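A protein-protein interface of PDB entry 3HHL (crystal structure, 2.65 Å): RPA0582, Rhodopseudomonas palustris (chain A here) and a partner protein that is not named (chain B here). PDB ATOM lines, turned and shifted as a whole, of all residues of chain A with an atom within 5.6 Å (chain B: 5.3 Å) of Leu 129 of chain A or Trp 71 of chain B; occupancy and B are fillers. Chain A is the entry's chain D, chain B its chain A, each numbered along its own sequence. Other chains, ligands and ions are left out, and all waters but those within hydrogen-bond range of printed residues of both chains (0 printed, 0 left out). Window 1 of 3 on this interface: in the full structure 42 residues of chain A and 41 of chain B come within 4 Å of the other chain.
A ring nitrogen (ND1) of His 26 of chain A lies within hydrogen-bond range of the indole nitrogen (NE1) of Trp 71 of chain B (2.9 Å).
The backbone NH of Gln 74 of chain B sits at hydrogen-bond distance from the backbone carbonyl oxygen of Lys 130 of chain A, 2.9 Å away.
The guanidinium group (NE) of Arg 21 of chain A is in salt-bridge range of the side-chain carboxylate (OE2) of Glu 76 of chain B, at 2.7 Å.
The side-chain carboxylate (OE1) of Glu 76 of chain B is in salt-bridge range of the guanidinium group (NE) of Arg 128 of chain A (2.8 Å).
The backbone carbonyl oxygen (O) of Trp 71 of chain B is in hydrogen-bond range of the backbone NH (N) of Ile 92 of chain B, at 2.8 Å.
N of Gly 73 of chain B is in hydrogen-bond range of O of Val 90 of chain B (3.0 Å).
The guanidinium group (NH1) of Arg 21 of chain A is in hydrogen-bond range of the backbone carbonyl oxygen (O) of Pro 24 of chain A (2.9 Å).
O of His 26 of chain A lies within hydrogen-bond range of N of Leu 129 of chain A, 2.8 Å away.
The backbone carbonyl oxygen of Leu 28 of chain A sits at hydrogen-bond distance from the backbone NH of Ile 127 of chain A (2.8 Å).
Among the printed residues, pairs that only touch across the chains: Ile 92 of chain A with Trp 71 of chain B (3.4 Å), Ile 127 of chain A with Phe 75 of chain B (3.7 Å), Arg 128 of chain A with Phe 75 of chain B (3.8 Å), Leu 129 of chain A with Trp 71 of chain B (3.8 Å), Leu 129 of chain A with Gly 73 of chain B (3.9 Å), Leu 129 of chain A with Gln 74 of chain B (3.3 Å), Leu 129 of chain A with Glu 76 of chain B (3.7 Å), Leu 129 of chain A with Val 90 of chain B (3.6 Å), Lys 130 of chain A with Gly 73 of chain B (3.4 Å), Lys 130 of chain A with Glu 76 of chain B (3.5 Å), Pro 131 of chain A with Gln 72 of chain B (3.9 Å), Pro 134 of chain A with Val 69 of chain B (3.6 Å) and Pro 134 of chain A with Gln 72 of chain B (3.6 Å).
Of chain B, only Trp 71, Gly 73, Gln 74, Glu 76 and Val 90 come within 4 Å of Leu 129 of chain A.
Of chain A, only His 26, Ile 92 and Leu 129 come within 4 Å of Trp 71 of chain B.
Of the printed residues of chain A, Gly 73 of chain B touches Leu 129 and Lys 130.
Of the printed residues of chain B, Arg 21 of chain A touches Glu 76.
Of the printed residues of chain A, Val 90 of chain B touches Leu 129.
Of the printed residues of chain A, Val 69 of chain B touches Pro 134.
Of the printed residues of chain B, Lys 130 of chain A touches Gly 73, Gln 74 and Glu 76.
Pro 24 of chain A touches none of the printed residues of chain B.
Leu 28 of chain A touches none of the printed residues of chain B.
The nearest residue of chain B that does not touch Leu 129 of chain A is Phe 75 of chain B (4.03 Å).
The nearest residue of chain A that does not touch Trp 71 of chain B is Leu 28 of chain A (4.6 Å).
The nearest printed residue of chain B that does not touch Pro 131 of chain A is Gly 73 of chain B (4.5 Å).
Hydrophobic or aromatic side chains of chain A that line the printed part of chain B: His 26, Ile 92, Ile 127, Leu 129 and Pro 134.
Printed residues of chain B that touch a printed residue of chain A: Val 69, Trp 71, Gln 72, Gly 73, Gln 74, Phe 75, Glu 76 and Val 90.
Along chain B the printed residues that touch a printed residue of chain A span positions 69 to 90.
Among the printed residues, 17 pairs touch across the chains.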
ATOM      1  N   ARG A  21     -26.010   1.781 -35.764  1.00  0.00           N
ATOM      2  CA  ARG A  21     -25.749   2.590 -36.973  1.00  0.00           C
ATOM      3  C   ARG A  21     -24.251   2.760 -37.157  1.00  0.00           C
ATOM      4  O   ARG A  21     -23.500   2.917 -36.197  1.00  0.00           O
ATOM      5  CB  ARG A  21     -26.477   3.957 -36.919  1.00  0.00           C
ATOM      6  CG  ARG A  21     -25.807   5.070 -36.089  1.00  0.00           C
ATOM      7  CD  ARG A  21     -25.552   4.755 -34.602  1.00  0.00           C
ATOM      8  NE  ARG A  21     -24.827   5.841 -33.927  1.00  0.00           N
ATOM      9  CZ  ARG A  21     -23.505   6.052 -33.993  1.00  0.00           C
ATOM     10  NH1 ARG A  21     -22.960   7.046 -33.323  1.00  0.00           N
ATOM     11  NH2 ARG A  21     -22.717   5.275 -34.723  1.00  0.00           N
ATOM     12  N   PRO A  24     -18.641   6.426 -35.716  1.00  0.00           N
ATOM     13  CA  PRO A  24     -18.072   6.490 -34.418  1.00  0.00           C
ATOM     14  C   PRO A  24     -19.137   6.840 -33.417  1.00  0.00           C
ATOM     15  O   PRO A  24     -20.142   7.477 -33.781  1.00  0.00           O
ATOM     16  CB  PRO A  24     -17.096   7.690 -34.515  1.00  0.00           C
ATOM     17  CG  PRO A  24     -16.803   7.836 -35.876  1.00  0.00           C
ATOM     18  CD  PRO A  24     -17.964   7.341 -36.657  1.00  0.00           C
ATOM     19  N   ILE A  25     -18.872   6.426 -32.187  1.00  0.00           N
ATOM     20  CA  ILE A  25     -19.667   6.717 -31.043  1.00  0.00           C
ATOM     21  C   ILE A  25     -18.720   7.397 -30.074  1.00  0.00           C
ATOM     22  O   ILE A  25     -17.570   7.011 -29.979  1.00  0.00           O
ATOM     23  CB  ILE A  25     -20.280   5.463 -30.400  1.00  0.00           C
ATOM     24  CG1 ILE A  25     -19.220   4.425 -30.039  1.00  0.00           C
ATOM     25  CG2 ILE A  25     -21.265   4.837 -31.369  1.00  0.00           C
ATOM     26  CD1 ILE A  25     -19.740   3.266 -29.138  1.00  0.00           C
ATOM     27  N   HIS A  26     -19.206   8.454 -29.433  1.00  0.00           N
ATOM     28  CA  HIS A  26     -18.502   9.152 -28.389  1.00  0.00           C
ATOM     29  C   HIS A  26     -19.201   8.854 -27.088  1.00  0.00           C
ATOM     30  O   HIS A  26     -20.433   8.965 -26.992  1.00  0.00           O
ATOM     31  CB  HIS A  26     -18.505  10.652 -28.630  1.00  0.00           C
ATOM     32  CG  HIS A  26     -17.466  11.089 -29.604  1.00  0.00           C
ATOM     33  ND1 HIS A  26     -17.245  12.413 -29.911  1.00  0.00           N
ATOM     34  CD2 HIS A  26     -16.614  10.369 -30.378  1.00  0.00           C
ATOM     35  CE1 HIS A  26     -16.290  12.487 -30.821  1.00  0.00           C
ATOM     36  NE2 HIS A  26     -15.877  11.264 -31.114  1.00  0.00           N
ATOM     37  N   MET A  27     -18.399   8.465 -26.115  1.00  0.00           N
ATOM     38  CA  MET A  27     -18.856   8.064 -24.828  1.00  0.00           C
ATOM     39  C   MET A  27     -18.386   9.114 -23.818  1.00  0.00           C
ATOM     40  O   MET A  27     -17.196   9.184 -23.457  1.00  0.00           O
ATOM     41  CB  MET A  27     -18.263   6.711 -24.498  1.00  0.00           C
ATOM     42  CG  MET A  27     -18.611   5.634 -25.490  1.00  0.00           C
ATOM     43  SD  MET A  27     -20.514   5.389 -25.788  1.00  0.00           S
ATOM     44  CE  MET A  27     -20.929   4.378 -24.194  1.00  0.00           C
ATOM     45  N   LEU A  28     -19.330   9.935 -23.380  1.00  0.00           N
ATOM     46  CA  LEU A  28     -19.053  10.949 -22.354  1.00  0.00           C
ATOM     47  C   LEU A  28     -19.202  10.280 -20.994  1.00  0.00           C
ATOM     48  O   LEU A  28     -20.284   9.753 -20.680  1.00  0.00           O
ATOM     49  CB  LEU A  28     -20.003  12.121 -22.499  1.00  0.00           C
ATOM     50  CG  LEU A  28     -19.977  13.202 -21.428  1.00  0.00           C
ATOM     51  CD1 LEU A  28     -18.598  13.866 -21.235  1.00  0.00           C
ATOM     52  CD2 LEU A  28     -21.054  14.256 -21.787  1.00  0.00           C
ATOM     53  N   ILE A  92     -14.205  12.069 -22.759  1.00  0.00           N
ATOM     54  CA  ILE A  92     -14.920  11.475 -23.879  1.00  0.00           C
ATOM     55  C   ILE A  92     -14.036  10.453 -24.547  1.00  0.00           C
ATOM     56  O   ILE A  92     -12.912  10.766 -24.927  1.00  0.00           O
ATOM     57  CB  ILE A  92     -15.376  12.535 -24.925  1.00  0.00           C
ATOM     58  CG1 ILE A  92     -16.401  13.523 -24.295  1.00  0.00           C
ATOM     59  CG2 ILE A  92     -15.952  11.841 -26.149  1.00  0.00           C
ATOM     60  CD1 ILE A  92     -16.701  14.768 -25.200  1.00  0.00           C
ATOM     61  N   ILE A 127     -22.742   8.522 -21.179  1.00  0.00           N
ATOM     62  CA  ILE A 127     -23.684   9.044 -22.152  1.00  0.00           C
ATOM     63  C   ILE A 127     -23.189   8.731 -23.542  1.00  0.00           C
ATOM     64  O   ILE A 127     -22.049   9.064 -23.888  1.00  0.00           O
ATOM     65  CB  ILE A 127     -23.834  10.561 -21.998  1.00  0.00           C
ATOM     66  CG1 ILE A 127     -24.167  10.894 -20.517  1.00  0.00           C
ATOM     67  CG2 ILE A 127     -24.884  11.089 -22.955  1.00  0.00           C
ATOM     68  CD1 ILE A 127     -24.333  12.376 -20.222  1.00  0.00           C
ATOM     69  N   ARG A 128     -24.038   8.092 -24.337  1.00  0.00           N
ATOM     70  CA  ARG A 128     -23.661   7.735 -25.674  1.00  0.00           C
ATOM     71  C   ARG A 128     -24.083   8.842 -26.610  1.00  0.00           C
ATOM     72  O   ARG A 128     -25.260   9.202 -26.608  1.00  0.00           O
ATOM     73  CB  ARG A 128     -24.325   6.458 -26.109  1.00  0.00           C
ATOM     74  CG  ARG A 128     -23.926   6.049 -27.533  1.00  0.00           C
ATOM     75  CD  ARG A 128     -24.799   4.906 -28.020  1.00  0.00           C
ATOM     76  NE  ARG A 128     -24.946   4.899 -29.452  1.00  0.00           N
ATOM     77  CZ  ARG A 128     -25.274   3.851 -30.179  1.00  0.00           C
ATOM     78  NH1 ARG A 128     -25.501   2.685 -29.618  1.00  0.00           N
ATOM     79  NH2 ARG A 128     -25.372   3.981 -31.494  1.00  0.00           N
ATOM     80  N   LEU A 129     -23.132   9.353 -27.420  1.00  0.00           N
ATOM     81  CA  LEU A 129     -23.435  10.388 -28.408  1.00  0.00           C
ATOM     82  C   LEU A 129     -22.917  10.073 -29.794  1.00  0.00           C
ATOM     83  O   LEU A 129     -21.900   9.405 -29.941  1.00  0.00           O
ATOM     84  CB  LEU A 129     -22.842  11.716 -27.967  1.00  0.00           C
ATOM     85  CG  LEU A 129     -23.247  12.150 -26.545  1.00  0.00           C
ATOM     86  CD1 LEU A 129     -22.032  12.055 -25.630  1.00  0.00           C
ATOM     87  CD2 LEU A 129     -23.872  13.536 -26.490  1.00  0.00           C
ATOM     88  N   LYS A 130     -23.618  10.560 -30.811  1.00  0.00           N
ATOM     89  CA  LYS A 130     -23.091  10.596 -32.158  1.00  0.00           C
ATOM     90  C   LYS A 130     -22.369  11.930 -32.330  1.00  0.00           C
ATOM     91  O   LYS A 130     -22.973  12.966 -32.168  1.00  0.00           O
ATOM     92  CB  LYS A 130     -24.205  10.539 -33.175  1.00  0.00           C
ATOM     93  CG  LYS A 130     -23.669  10.573 -34.605  1.00  0.00           C
ATOM     94  CD  LYS A 130     -24.621  11.143 -35.605  1.00  0.00           C
ATOM     95  CE  LYS A 130     -25.491  10.116 -36.249  1.00  0.00           C
ATOM     96  NZ  LYS A 130     -24.819   9.675 -37.519  1.00  0.00           N
ATOM     97  N   PRO A 131     -21.083  11.913 -32.669  1.00  0.00           N
ATOM     98  CA  PRO A 131     -20.386  13.174 -32.917  1.00  0.00           C
ATOM     99  C   PRO A 131     -21.019  14.014 -34.030  1.00  0.00           C
ATOM    100  O   PRO A 131     -21.423  13.472 -35.029  1.00  0.00           O
ATOM    101  CB  PRO A 131     -18.981  12.732 -33.352  1.00  0.00           C
ATOM    102  CG  PRO A 131     -18.888  11.354 -33.023  1.00  0.00           C
ATOM    103  CD  PRO A 131     -20.258  10.772 -33.041  1.00  0.00           C
ATOM    104  N   PRO A 134     -19.338  20.604 -35.252  1.00  0.00           N
ATOM    105  CA  PRO A 134     -19.766  21.772 -34.438  1.00  0.00           C
ATOM    106  C   PRO A 134     -20.261  23.019 -35.253  1.00  0.00           C
ATOM    107  O   PRO A 134     -19.584  24.047 -35.318  1.00  0.00           O
ATOM    108  CB  PRO A 134     -18.513  22.098 -33.604  1.00  0.00           C
ATOM    109  CG  PRO A 134     -17.425  21.093 -34.024  1.00  0.00           C
ATOM    110  CD  PRO A 134     -18.101  19.989 -34.713  1.00  0.00           C
ATOM    111  N   LEU B  28     -18.815  22.359 -20.369  1.00  0.00           N
ATOM    112  CA  LEU B  28     -19.662  21.239 -20.810  1.00  0.00           C
ATOM    113  C   LEU B  28     -21.111  21.558 -20.497  1.00  0.00           C
ATOM    114  O   LEU B  28     -21.471  21.734 -19.338  1.00  0.00           O
ATOM    115  CB  LEU B  28     -19.227  19.943 -20.163  1.00  0.00           C
ATOM    116  CG  LEU B  28     -20.040  18.682 -20.419  1.00  0.00           C
ATOM    117  CD1 LEU B  28     -20.183  18.321 -21.890  1.00  0.00           C
ATOM    118  CD2 LEU B  28     -19.390  17.530 -19.608  1.00  0.00           C
ATOM    119  N   VAL B  69     -17.545  26.667 -29.970  1.00  0.00           N
ATOM    120  CA  VAL B  69     -17.943  25.319 -29.703  1.00  0.00           C
ATOM    121  C   VAL B  69     -16.885  24.425 -30.250  1.00  0.00           C
ATOM    122  O   VAL B  69     -16.706  24.405 -31.449  1.00  0.00           O
ATOM    123  CB  VAL B  69     -19.267  24.976 -30.418  1.00  0.00           C
ATOM    124  CG1 VAL B  69     -19.563  23.476 -30.263  1.00  0.00           C
ATOM    125  CG2 VAL B  69     -20.399  25.816 -29.821  1.00  0.00           C
ATOM    126  N   VAL B  70     -16.218  23.665 -29.380  1.00  0.00           N
ATOM    127  CA  VAL B  70     -15.128  22.761 -29.788  1.00  0.00           C
ATOM    128  C   VAL B  70     -15.518  21.299 -29.882  1.00  0.00           C
ATOM    129  O   VAL B  70     -14.759  20.508 -30.397  1.00  0.00           O
ATOM    130  CB  VAL B  70     -13.933  22.836 -28.811  1.00  0.00           C
ATOM    131  CG1 VAL B  70     -13.324  24.233 -28.836  1.00  0.00           C
ATOM    132  CG2 VAL B  70     -14.364  22.420 -27.410  1.00  0.00           C
ATOM    133  N   TRP B  71     -16.685  20.919 -29.375  1.00  0.00           N
ATOM    134  CA  TRP B  71     -17.210  19.547 -29.554  1.00  0.00           C
ATOM    135  C   TRP B  71     -18.684  19.568 -29.339  1.00  0.00           C
ATOM    136  O   TRP B  71     -19.189  20.284 -28.501  1.00  0.00           O
ATOM    137  CB  TRP B  71     -16.595  18.551 -28.558  1.00  0.00           C
ATOM    138  CG  TRP B  71     -17.296  17.213 -28.486  1.00  0.00           C
ATOM    139  CD1 TRP B  71     -17.060  16.145 -29.265  1.00  0.00           C
ATOM    140  CD2 TRP B  71     -18.328  16.821 -27.582  1.00  0.00           C
ATOM    141  NE1 TRP B  71     -17.889  15.104 -28.931  1.00  0.00           N
ATOM    142  CE2 TRP B  71     -18.680  15.494 -27.899  1.00  0.00           C
ATOM    143  CE3 TRP B  71     -18.988  17.458 -26.554  1.00  0.00           C
ATOM    144  CZ2 TRP B  71     -19.642  14.786 -27.218  1.00  0.00           C
ATOM    145  CZ3 TRP B  71     -19.961  16.760 -25.873  1.00  0.00           C
ATOM    146  CH2 TRP B  71     -20.281  15.421 -26.212  1.00  0.00           C
ATOM    147  N   GLN B  72     -19.383  18.736 -30.079  1.00  0.00           N
ATOM    148  CA  GLN B  72     -20.823  18.708 -29.958  1.00  0.00           C
ATOM    149  C   GLN B  72     -21.303  17.308 -30.327  1.00  0.00           C
ATOM    150  O   GLN B  72     -20.760  16.706 -31.257  1.00  0.00           O
ATOM    151  CB  GLN B  72     -21.402  19.741 -30.921  1.00  0.00           C
ATOM    152  CG  GLN B  72     -22.909  19.806 -30.889  1.00  0.00           C
ATOM    153  CD  GLN B  72     -23.508  21.036 -31.604  1.00  0.00           C
ATOM    154  OE1 GLN B  72     -24.709  21.289 -31.465  1.00  0.00           O
ATOM    155  NE2 GLN B  72     -22.685  21.790 -32.360  1.00  0.00           N
ATOM    156  N   GLY B  73     -22.298  16.793 -29.606  1.00  0.00           N
ATOM    157  CA  GLY B  73     -22.837  15.471 -29.910  1.00  0.00           C
ATOM    158  C   GLY B  73     -24.332  15.372 -29.850  1.00  0.00           C
ATOM    159  O   GLY B  73     -24.968  16.122 -29.136  1.00  0.00           O
ATOM    160  N   GLN B  74     -24.886  14.434 -30.608  1.00  0.00           N
ATOM    161  CA  GLN B  74     -26.308  14.106 -30.537  1.00  0.00           C
ATOM    162  C   GLN B  74     -26.528  12.974 -29.554  1.00  0.00           C
ATOM    163  O   GLN B  74     -26.022  11.905 -29.737  1.00  0.00           O
ATOM    164  CB  GLN B  74     -26.830  13.740 -31.914  1.00  0.00           C
ATOM    165  CG  GLN B  74     -28.252  13.246 -31.994  1.00  0.00           C
ATOM    166  CD  GLN B  74     -28.577  12.742 -33.443  1.00  0.00           C
ATOM    167  OE1 GLN B  74     -28.388  13.495 -34.415  1.00  0.00           O
ATOM    168  NE2 GLN B  74     -29.015  11.471 -33.588  1.00  0.00           N
ATOM    169  N   PHE B  75     -27.335  13.211 -28.534  1.00  0.00           N
ATOM    170  CA  PHE B  75     -27.612  12.242 -27.500  1.00  0.00           C
ATOM    171  C   PHE B  75     -28.251  11.051 -28.108  1.00  0.00           C
ATOM    172  O   PHE B  75     -29.163  11.208 -28.884  1.00  0.00           O
ATOM    173  CB  PHE B  75     -28.537  12.867 -26.488  1.00  0.00           C
ATOM    174  CG  PHE B  75     -28.935  11.966 -25.398  1.00  0.00           C
ATOM    175  CD1 PHE B  75     -28.208  11.905 -24.240  1.00  0.00           C
ATOM    176  CD2 PHE B  75     -30.077  11.181 -25.506  1.00  0.00           C
ATOM    177  CE1 PHE B  75     -28.602  11.061 -23.183  1.00  0.00           C
ATOM    178  CE2 PHE B  75     -30.458  10.331 -24.458  1.00  0.00           C
ATOM    179  CZ  PHE B  75     -29.710  10.274 -23.297  1.00  0.00           C
ATOM    180  N   GLU B  76     -27.758   9.852 -27.776  1.00  0.00           N
ATOM    181  CA  GLU B  76     -28.337   8.583 -28.247  1.00  0.00           C
ATOM    182  C   GLU B  76     -28.795   7.644 -27.125  1.00  0.00           C
ATOM    183  O   GLU B  76     -29.741   6.902 -27.297  1.00  0.00           O
ATOM    184  CB  GLU B  76     -27.311   7.859 -29.152  1.00  0.00           C
ATOM    185  CG  GLU B  76     -27.081   8.521 -30.513  1.00  0.00           C
ATOM    186  CD  GLU B  76     -26.096   7.788 -31.432  1.00  0.00           C
ATOM    187  OE1 GLU B  76     -25.036   7.326 -30.943  1.00  0.00           O
ATOM    188  OE2 GLU B  76     -26.359   7.727 -32.673  1.00  0.00           O
ATOM    189  N   VAL B  90     -25.904  18.665 -26.242  1.00  0.00           N
ATOM    190  CA  VAL B  90     -24.730  18.331 -25.465  1.00  0.00           C
ATOM    191  C   VAL B  90     -23.535  18.833 -26.208  1.00  0.00           C
ATOM    192  O   VAL B  90     -23.311  18.439 -27.328  1.00  0.00           O
ATOM    193  CB  VAL B  90     -24.566  16.847 -25.254  1.00  0.00           C
ATOM    194  CG1 VAL B  90     -23.323  16.571 -24.409  1.00  0.00           C
ATOM    195  CG2 VAL B  90     -25.755  16.311 -24.584  1.00  0.00           C
ATOM    196  N   PHE B  91     -22.765  19.713 -25.589  1.00  0.00           N
ATOM    197  CA  PHE B  91     -21.631  20.307 -26.283  1.00  0.00           C
ATOM    198  C   PHE B  91     -20.673  20.906 -25.294  1.00  0.00           C
ATOM    199  O   PHE B  91     -21.040  21.168 -24.105  1.00  0.00           O
ATOM    200  CB  PHE B  91     -22.081  21.389 -27.280  1.00  0.00           C
ATOM    201  CG  PHE B  91     -22.765  22.538 -26.652  1.00  0.00           C
ATOM    202  CD1 PHE B  91     -24.107  22.494 -26.398  1.00  0.00           C
ATOM    203  CD2 PHE B  91     -22.054  23.665 -26.279  1.00  0.00           C
ATOM    204  CE1 PHE B  91     -24.761  23.593 -25.777  1.00  0.00           C
ATOM    205  CE2 PHE B  91     -22.667  24.763 -25.633  1.00  0.00           C
ATOM    206  CZ  PHE B  91     -24.024  24.729 -25.387  1.00  0.00           C
ATOM    207  N   ILE B  92     -19.461  21.150 -25.808  1.00  0.00           N
ATOM    208  CA  ILE B  92     -18.421  21.830 -25.047  1.00  0.00           C
ATOM    209  C   ILE B  92     -18.051  23.116 -25.728  1.00  0.00           C
ATOM    210  O   ILE B  92     -17.745  23.122 -26.897  1.00  0.00           O
ATOM    211  CB  ILE B  92     -17.164  20.970 -24.841  1.00  0.00           C
ATOM    212  CG1 ILE B  92     -17.489  19.728 -23.969  1.00  0.00           C
ATOM    213  CG2 ILE B  92     -16.027  21.841 -24.238  1.00  0.00           C
ATOM    214  CD1 ILE B  92     -16.370  18.613 -24.050  1.00  0.00           C
